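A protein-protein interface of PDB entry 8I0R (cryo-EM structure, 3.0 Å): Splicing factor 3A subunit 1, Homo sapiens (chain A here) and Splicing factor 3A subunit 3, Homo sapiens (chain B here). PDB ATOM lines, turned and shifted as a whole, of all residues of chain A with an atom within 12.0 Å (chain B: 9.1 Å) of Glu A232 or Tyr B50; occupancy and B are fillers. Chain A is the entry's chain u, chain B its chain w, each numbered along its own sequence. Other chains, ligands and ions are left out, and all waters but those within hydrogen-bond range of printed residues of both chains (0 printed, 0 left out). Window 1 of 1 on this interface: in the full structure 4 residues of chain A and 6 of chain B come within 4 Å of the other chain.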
ATOM      1  N   PRO A 222      17.068   9.866 -26.994  1.00  0.00           N
ATOM      2  CA  PRO A 222      16.215  10.968 -26.526  1.00  0.00           C
ATOM      3  C   PRO A 222      16.140  11.112 -25.015  1.00  0.00           C
ATOM      4  O   PRO A 222      15.494  12.051 -24.536  1.00  0.00           O
ATOM      5  CB  PRO A 222      14.844  10.587 -27.094  1.00  0.00           C
ATOM      6  CG  PRO A 222      14.836   9.129 -27.007  1.00  0.00           C
ATOM      7  CD  PRO A 222      16.237   8.710 -27.392  1.00  0.00           C
ATOM      8  N   LYS A 223      16.789  10.226 -24.258  1.00  0.00           N
ATOM      9  CA  LYS A 223      16.703  10.270 -22.805  1.00  0.00           C
ATOM     10  C   LYS A 223      17.498  11.417 -22.197  1.00  0.00           C
ATOM     11  O   LYS A 223      17.384  11.656 -20.990  1.00  0.00           O
ATOM     12  N   SER A 227      20.648  15.065 -27.412  1.00  0.00           N
ATOM     13  CA  SER A 227      19.580  15.820 -28.053  1.00  0.00           C
ATOM     14  C   SER A 227      18.587  16.285 -26.995  1.00  0.00           C
ATOM     15  O   SER A 227      18.609  15.827 -25.848  1.00  0.00           O
ATOM     16  N   LYS A 228      17.702  17.197 -27.395  1.00  0.00           N
ATOM     17  CA  LYS A 228      16.678  17.741 -26.510  1.00  0.00           C
ATOM     18  C   LYS A 228      15.310  17.546 -27.146  1.00  0.00           C
ATOM     19  O   LYS A 228      15.109  17.893 -28.314  1.00  0.00           O
ATOM     20  N   LEU A 229      14.376  16.993 -26.378  1.00  0.00           N
ATOM     21  CA  LEU A 229      12.990  16.864 -26.807  1.00  0.00           C
ATOM     22  C   LEU A 229      12.193  18.023 -26.221  1.00  0.00           C
ATOM     23  O   LEU A 229      12.238  18.259 -25.010  1.00  0.00           O
ATOM     24  N   LYS A 230      11.464  18.741 -27.078  1.00  0.00           N
ATOM     25  CA  LYS A 230      10.721  19.923 -26.664  1.00  0.00           C
ATOM     26  C   LYS A 230       9.215  19.814 -26.836  1.00  0.00           C
ATOM     27  O   LYS A 230       8.494  20.675 -26.321  1.00  0.00           O
ATOM     28  N   LYS A 231       8.718  18.789 -27.530  1.00  0.00           N
ATOM     29  CA  LYS A 231       7.279  18.560 -27.598  1.00  0.00           C
ATOM     30  C   LYS A 231       6.726  18.080 -26.265  1.00  0.00           C
ATOM     31  O   LYS A 231       5.503  18.031 -26.084  1.00  0.00           O
ATOM     32  N   GLU A 232       7.603  17.711 -25.333  1.00  0.00           N
ATOM     33  CA  GLU A 232       7.216  17.461 -23.956  1.00  0.00           C
ATOM     34  C   GLU A 232       7.435  18.670 -23.059  1.00  0.00           C
ATOM     35  O   GLU A 232       6.596  18.936 -22.189  1.00  0.00           O
ATOM     36  N   ALA A 233       8.523  19.416 -23.261  1.00  0.00           N
ATOM     37  CA  ALA A 233       8.870  20.542 -22.405  1.00  0.00           C
ATOM     38  C   ALA A 233       8.142  21.834 -22.750  1.00  0.00           C
ATOM     39  O   ALA A 233       8.234  22.799 -21.984  1.00  0.00           O
ATOM     40  N   GLU A 234       7.461  21.900 -23.898  1.00  0.00           N
ATOM     41  CA  GLU A 234       6.647  23.070 -24.206  1.00  0.00           C
ATOM     42  C   GLU A 234       5.348  22.720 -24.924  1.00  0.00           C
ATOM     43  O   GLU A 234       4.839  23.546 -25.692  1.00  0.00           O
ATOM     44  N   ASN A 235       4.785  21.533 -24.701  1.00  0.00           N
ATOM     45  CA  ASN A 235       3.765  20.989 -25.597  1.00  0.00           C
ATOM     46  C   ASN A 235       2.467  20.624 -24.894  1.00  0.00           C
ATOM     47  O   ASN A 235       2.292  19.486 -24.436  1.00  0.00           O
ATOM     48  N   PRO A 236       1.512  21.555 -24.824  1.00  0.00           N
ATOM     49  CA  PRO A 236       0.152  21.169 -24.415  1.00  0.00           C
ATOM     50  C   PRO A 236      -0.530  20.261 -25.423  1.00  0.00           C
ATOM     51  O   PRO A 236      -1.344  19.420 -25.024  1.00  0.00           O
ATOM     52  CB  PRO A 236      -0.581  22.514 -24.286  1.00  0.00           C
ATOM     53  CG  PRO A 236       0.496  23.562 -24.281  1.00  0.00           C
ATOM     54  CD  PRO A 236       1.630  23.001 -25.069  1.00  0.00           C
ATOM     55  N   ARG A 237      -0.199  20.376 -26.709  1.00  0.00           N
ATOM     56  CA  ARG A 237      -0.777  19.481 -27.704  1.00  0.00           C
ATOM     57  C   ARG A 237      -0.329  18.046 -27.464  1.00  0.00           C
ATOM     58  O   ARG A 237      -1.156  17.127 -27.411  1.00  0.00           O
ATOM     59  N   GLU A 238       0.982  17.840 -27.307  1.00  0.00           N
ATOM     60  CA  GLU A 238       1.499  16.510 -27.001  1.00  0.00           C
ATOM     61  C   GLU A 238       1.018  16.030 -25.638  1.00  0.00           C
ATOM     62  O   GLU A 238       0.765  14.835 -25.451  1.00  0.00           O
ATOM     63  N   VAL A 239       0.876  16.945 -24.676  1.00  0.00           N
ATOM     64  CA  VAL A 239       0.402  16.555 -23.351  1.00  0.00           C
ATOM     65  C   VAL A 239      -1.021  16.019 -23.424  1.00  0.00           C
ATOM     66  O   VAL A 239      -1.329  14.953 -22.875  1.00  0.00           O
ATOM     67  N   LEU A 240      -1.908  16.738 -24.118  1.00  0.00           N
ATOM     68  CA  LEU A 240      -3.286  16.283 -24.262  1.00  0.00           C
ATOM     69  C   LEU A 240      -3.354  14.988 -25.058  1.00  0.00           C
ATOM     70  O   LEU A 240      -4.099  14.068 -24.692  1.00  0.00           O
ATOM     71  N   ASP A 241      -2.583  14.897 -26.147  1.00  0.00           N
ATOM     72  CA  ASP A 241      -2.520  13.656 -26.911  1.00  0.00           C
ATOM     73  C   ASP A 241      -2.148  12.473 -26.025  1.00  0.00           C
ATOM     74  O   ASP A 241      -2.905  11.501 -25.930  1.00  0.00           O
ATOM     75  N   GLN A 242      -0.992  12.547 -25.355  1.00  0.00           N
ATOM     76  CA  GLN A 242      -0.511  11.425 -24.553  1.00  0.00           C
ATOM     77  C   GLN A 242      -1.435  11.124 -23.379  1.00  0.00           C
ATOM     78  O   GLN A 242      -1.571   9.963 -22.979  1.00  0.00           O
ATOM     79  N   VAL A 243      -2.092  12.145 -22.821  1.00  0.00           N
ATOM     80  CA  VAL A 243      -2.979  11.908 -21.684  1.00  0.00           C
ATOM     81  C   VAL A 243      -4.237  11.174 -22.129  1.00  0.00           C
ATOM     82  O   VAL A 243      -4.657  10.189 -21.503  1.00  0.00           O
ATOM     83  N   TYR B  11      13.534  13.921 -13.813  1.00  0.00           N
ATOM     84  CA  TYR B  11      12.590  14.412 -14.807  1.00  0.00           C
ATOM     85  C   TYR B  11      11.671  13.302 -15.302  1.00  0.00           C
ATOM     86  O   TYR B  11      10.481  13.537 -15.533  1.00  0.00           O
ATOM     87  N   HIS B  12      12.193  12.082 -15.453  1.00  0.00           N
ATOM     88  CA  HIS B  12      11.371  10.986 -15.947  1.00  0.00           C
ATOM     89  C   HIS B  12      10.288  10.619 -14.948  1.00  0.00           C
ATOM     90  O   HIS B  12       9.129  10.426 -15.327  1.00  0.00           O
ATOM     91  N   GLU B  14       9.038  12.592 -12.498  1.00  0.00           N
ATOM     92  CA  GLU B  14       8.100  13.710 -12.419  1.00  0.00           C
ATOM     93  C   GLU B  14       7.171  13.740 -13.628  1.00  0.00           C
ATOM     94  O   GLU B  14       5.964  13.969 -13.493  1.00  0.00           O
ATOM     95  N   LYS B  15       7.709  13.468 -14.820  1.00  0.00           N
ATOM     96  CA  LYS B  15       6.907  13.560 -16.032  1.00  0.00           C
ATOM     97  C   LYS B  15       5.958  12.381 -16.159  1.00  0.00           C
ATOM     98  O   LYS B  15       4.833  12.537 -16.641  1.00  0.00           O
ATOM     99  N   GLU B  16       6.392  11.192 -15.738  1.00  0.00           N
ATOM    100  CA  GLU B  16       5.486  10.052 -15.707  1.00  0.00           C
ATOM    101  C   GLU B  16       4.308  10.322 -14.783  1.00  0.00           C
ATOM    102  O   GLU B  16       3.149  10.110 -15.163  1.00  0.00           O
ATOM    103  N   ARG B  17       4.582  10.818 -13.573  1.00  0.00           N
ATOM    104  CA  ARG B  17       3.494  11.129 -12.650  1.00  0.00           C
ATOM    105  C   ARG B  17       2.595  12.235 -13.191  1.00  0.00           C
ATOM    106  O   ARG B  17       1.370  12.180 -13.029  1.00  0.00           O
ATOM    107  N   LEU B  18       3.175  13.234 -13.861  1.00  0.00           N
ATOM    108  CA  LEU B  18       2.372  14.336 -14.387  1.00  0.00           C
ATOM    109  C   LEU B  18       1.465  13.875 -15.523  1.00  0.00           C
ATOM    110  O   LEU B  18       0.270  14.202 -15.547  1.00  0.00           O
ATOM    111  N   MET B  19       2.020  13.136 -16.488  1.00  0.00           N
ATOM    112  CA  MET B  19       1.206  12.585 -17.564  1.00  0.00           C
ATOM    113  C   MET B  19       0.132  11.650 -17.024  1.00  0.00           C
ATOM    114  O   MET B  19      -1.008  11.669 -17.503  1.00  0.00           O
ATOM    115  N   ARG B  42      -6.205  23.126 -14.021  1.00  0.00           N
ATOM    116  CA  ARG B  42      -5.287  22.150 -13.446  1.00  0.00           C
ATOM    117  C   ARG B  42      -4.625  21.301 -14.524  1.00  0.00           C
ATOM    118  O   ARG B  42      -3.468  20.906 -14.379  1.00  0.00           O
ATOM    119  N   THR B  43      -5.349  20.983 -15.595  1.00  0.00           N
ATOM    120  CA  THR B  43      -4.754  20.226 -16.691  1.00  0.00           C
ATOM    121  C   THR B  43      -3.711  21.061 -17.419  1.00  0.00           C
ATOM    122  O   THR B  43      -2.642  20.555 -17.784  1.00  0.00           O
ATOM    123  N   ARG B  44      -4.005  22.346 -17.634  1.00  0.00           N
ATOM    124  CA  ARG B  44      -2.980  23.249 -18.149  1.00  0.00           C
ATOM    125  C   ARG B  44      -1.786  23.323 -17.202  1.00  0.00           C
ATOM    126  O   ARG B  44      -0.636  23.399 -17.643  1.00  0.00           O
ATOM    127  N   ALA B  45      -2.041  23.277 -15.890  1.00  0.00           N
ATOM    128  CA  ALA B  45      -0.959  23.329 -14.913  1.00  0.00           C
ATOM    129  C   ALA B  45      -0.129  22.048 -14.917  1.00  0.00           C
ATOM    130  O   ALA B  45       1.089  22.096 -14.732  1.00  0.00           O
ATOM    131  N   MET B  46      -0.772  20.894 -15.086  1.00  0.00           N
ATOM    132  CA  MET B  46      -0.037  19.639 -15.197  1.00  0.00           C
ATOM    133  C   MET B  46       0.797  19.610 -16.470  1.00  0.00           C
ATOM    134  O   MET B  46       1.938  19.130 -16.465  1.00  0.00           O
ATOM    135  N   GLN B  47       0.250  20.143 -17.567  1.00  0.00           N
ATOM    136  CA  GLN B  47       1.036  20.289 -18.787  1.00  0.00           C
ATOM    137  C   GLN B  47       2.191  21.265 -18.595  1.00  0.00           C
ATOM    138  O   GLN B  47       3.267  21.065 -19.162  1.00  0.00           O
ATOM    139  N   ASP B  48       2.004  22.294 -17.764  1.00  0.00           N
ATOM    140  CA  ASP B  48       3.083  23.243 -17.495  1.00  0.00           C
ATOM    141  C   ASP B  48       4.138  22.644 -16.572  1.00  0.00           C
ATOM    142  O   ASP B  48       5.318  22.989 -16.669  1.00  0.00           O
ATOM    143  N   ARG B  49       3.734  21.759 -15.659  1.00  0.00           N
ATOM    144  CA  ARG B  49       4.703  21.033 -14.842  1.00  0.00           C
ATOM    145  C   ARG B  49       5.540  20.096 -15.704  1.00  0.00           C
ATOM    146  O   ARG B  49       6.776  20.057 -15.584  1.00  0.00           O
ATOM    147  N   TYR B  50       4.879  19.329 -16.578  1.00  0.00           N
ATOM    148  CA  TYR B  50       5.604  18.515 -17.546  1.00  0.00           C
ATOM    149  C   TYR B  50       6.506  19.382 -18.413  1.00  0.00           C
ATOM    150  O   TYR B  50       7.635  18.994 -18.735  1.00  0.00           O
ATOM    151  N   MET B  51       6.039  20.582 -18.760  1.00  0.00           N
ATOM    152  CA  MET B  51       6.825  21.473 -19.601  1.00  0.00           C
ATOM    153  C   MET B  51       8.036  22.033 -18.870  1.00  0.00           C
ATOM    154  O   MET B  51       9.097  22.195 -19.476  1.00  0.00           O
ATOM    155  N   GLU B  52       7.906  22.333 -17.580  1.00  0.00           N
ATOM    156  CA  GLU B  52       9.053  22.809 -16.817  1.00  0.00           C
ATOM    157  C   GLU B  52      10.084  21.703 -16.640  1.00  0.00           C
ATOM    158  O   GLU B  52      11.291  21.941 -16.775  1.00  0.00           O
ATOM    159  N   VAL B  53       9.626  20.483 -16.349  1.00  0.00           N
ATOM    160  CA  VAL B  53      10.553  19.357 -16.281  1.00  0.00           C
ATOM    161  C   VAL B  53      11.264  19.174 -17.617  1.00  0.00           C
ATOM    162  O   VAL B  53      12.484  18.969 -17.666  1.00  0.00           O
ATOM    163  N   SER B  54      10.523  19.283 -18.723  1.00  0.00           N
ATOM    164  CA  SER B  54      11.122  19.079 -20.039  1.00  0.00           C
ATOM    165  C   SER B  54      12.070  20.214 -20.411  1.00  0.00           C
ATOM    166  O   SER B  54      13.072  19.992 -21.097  1.00  0.00           O
ATOM    167  N   GLY B  55      11.765  21.440 -19.982  1.00  0.00           N
ATOM    168  CA  GLY B  55      12.653  22.555 -20.255  1.00  0.00           C
ATOM    169  C   GLY B  55      13.929  22.494 -19.443  1.00  0.00           C
ATOM    170  O   GLY B  55      14.981  22.955 -19.897  1.00  0.00           O
ATOM    171  N   ASN B  56      13.854  21.941 -18.230  1.00  0.00           N
ATOM    172  CA  ASN B  56      15.067  21.682 -17.467  1.00  0.00           C
ATOM    173  C   ASN B  56      15.851  20.509 -18.042  1.00  0.00           C
ATOM    174  O   ASN B  56      17.077  20.450 -17.893  1.00  0.00           O
ATOM    175  N   LEU B  57      15.170  19.567 -18.700  1.00  0.00           N
ATOM    176  CA  LEU B  57      15.860  18.388 -19.211  1.00  0.00           C
ATOM    177  C   LEU B  57      16.478  18.600 -20.591  1.00  0.00           C
ATOM    178  O   LEU B  57      17.555  18.064 -20.868  1.00  0.00           O
ATOM    179  N   ARG B  58      15.824  19.366 -21.466  1.00  0.00           N
ATOM    180  CA  ARG B  58      16.292  19.498 -22.841  1.00  0.00           C
ATOM    181  C   ARG B  58      17.477  20.444 -22.976  1.00  0.00           C
ATOM    182  O   ARG B  58      18.059  20.535 -24.061  1.00  0.00           O
ATOM    183  N   GLU B 109       1.156  15.313  -8.579  1.00  0.00           N
ATOM    184  CA  GLU B 109       0.291  15.524  -9.739  1.00  0.00           C
ATOM    185  C   GLU B 109      -0.930  14.608  -9.739  1.00  0.00           C
ATOM    186  O   GLU B 109      -1.291  14.054 -10.780  1.00  0.00           O
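Printed residues of chain B that touch a printed residue of chain A: Tyr B50, Met B51, Ser B54, Gly B55 and Arg B58.
Among the printed residues, 6 pairs touch across the chains.
Among the printed residues, no Asp or Glu carboxylate lies within 4 Å of a Lys or Arg side-chain nitrogen of the other chain.
The backbone carbonyl oxygen of Met B51 lies close to the backbone carbonyl oxygen of Ala A233 (2.7 Å).
Printed residues of chain B within 4 Å of Lys A228: Arg B58 (3.96 Å).
No residue of chain B comes within 4 Å of Lys A230.
No residue of chain B comes within 4 Å of Lys A231.
Glu A232 touches just these residues of chain B: Tyr B50 (3.6 Å) and Met B51 (3.6 Å).
Ala A233 touches just these residues of chain B: Met B51 (2.7 Å), Ser B54 (3.6 Å) and Gly B55 (3.9 Å).
No residue of chain A comes within 4 Å of Lys B15.
No residue of chain A comes within 4 Å of Leu B18.
No residue of chain A comes within 4 Å of Met B46.
No residue of chain A comes within 4 Å of Gln B47.
No residue of chain A comes within 4 Å of Asp B48.
No residue of chain A comes within 4 Å of Arg B49.
Tyr B50 touches just one residue of chain A: Glu A232 (3.6 Å).
Met B51 touches two residues of chain A.
No residue of chain A comes within 4 Å of Glu B52.
No residue of chain A comes within 4 Å of Val B53.
Of the printed residues of chain A, Arg B58 touches Lys A228.
The nearest residue of chain B that does not touch Glu A232 is Ser B54 (4.8 Å).
The nearest residue of chain A that does not touch Tyr B50 is Ala A233 (4.2 Å).
The nearest printed residue of chain A that does not touch Gly B55 is Glu A234 (5.8 Å).
Lys A228 touches Arg B58.
Glu A232 touches Tyr B50.
Met B51 touches Glu A232.
Ala A233 touches Ser B54.
Ala A233 touches Gly B55 (CA to N, 3.9 Å).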
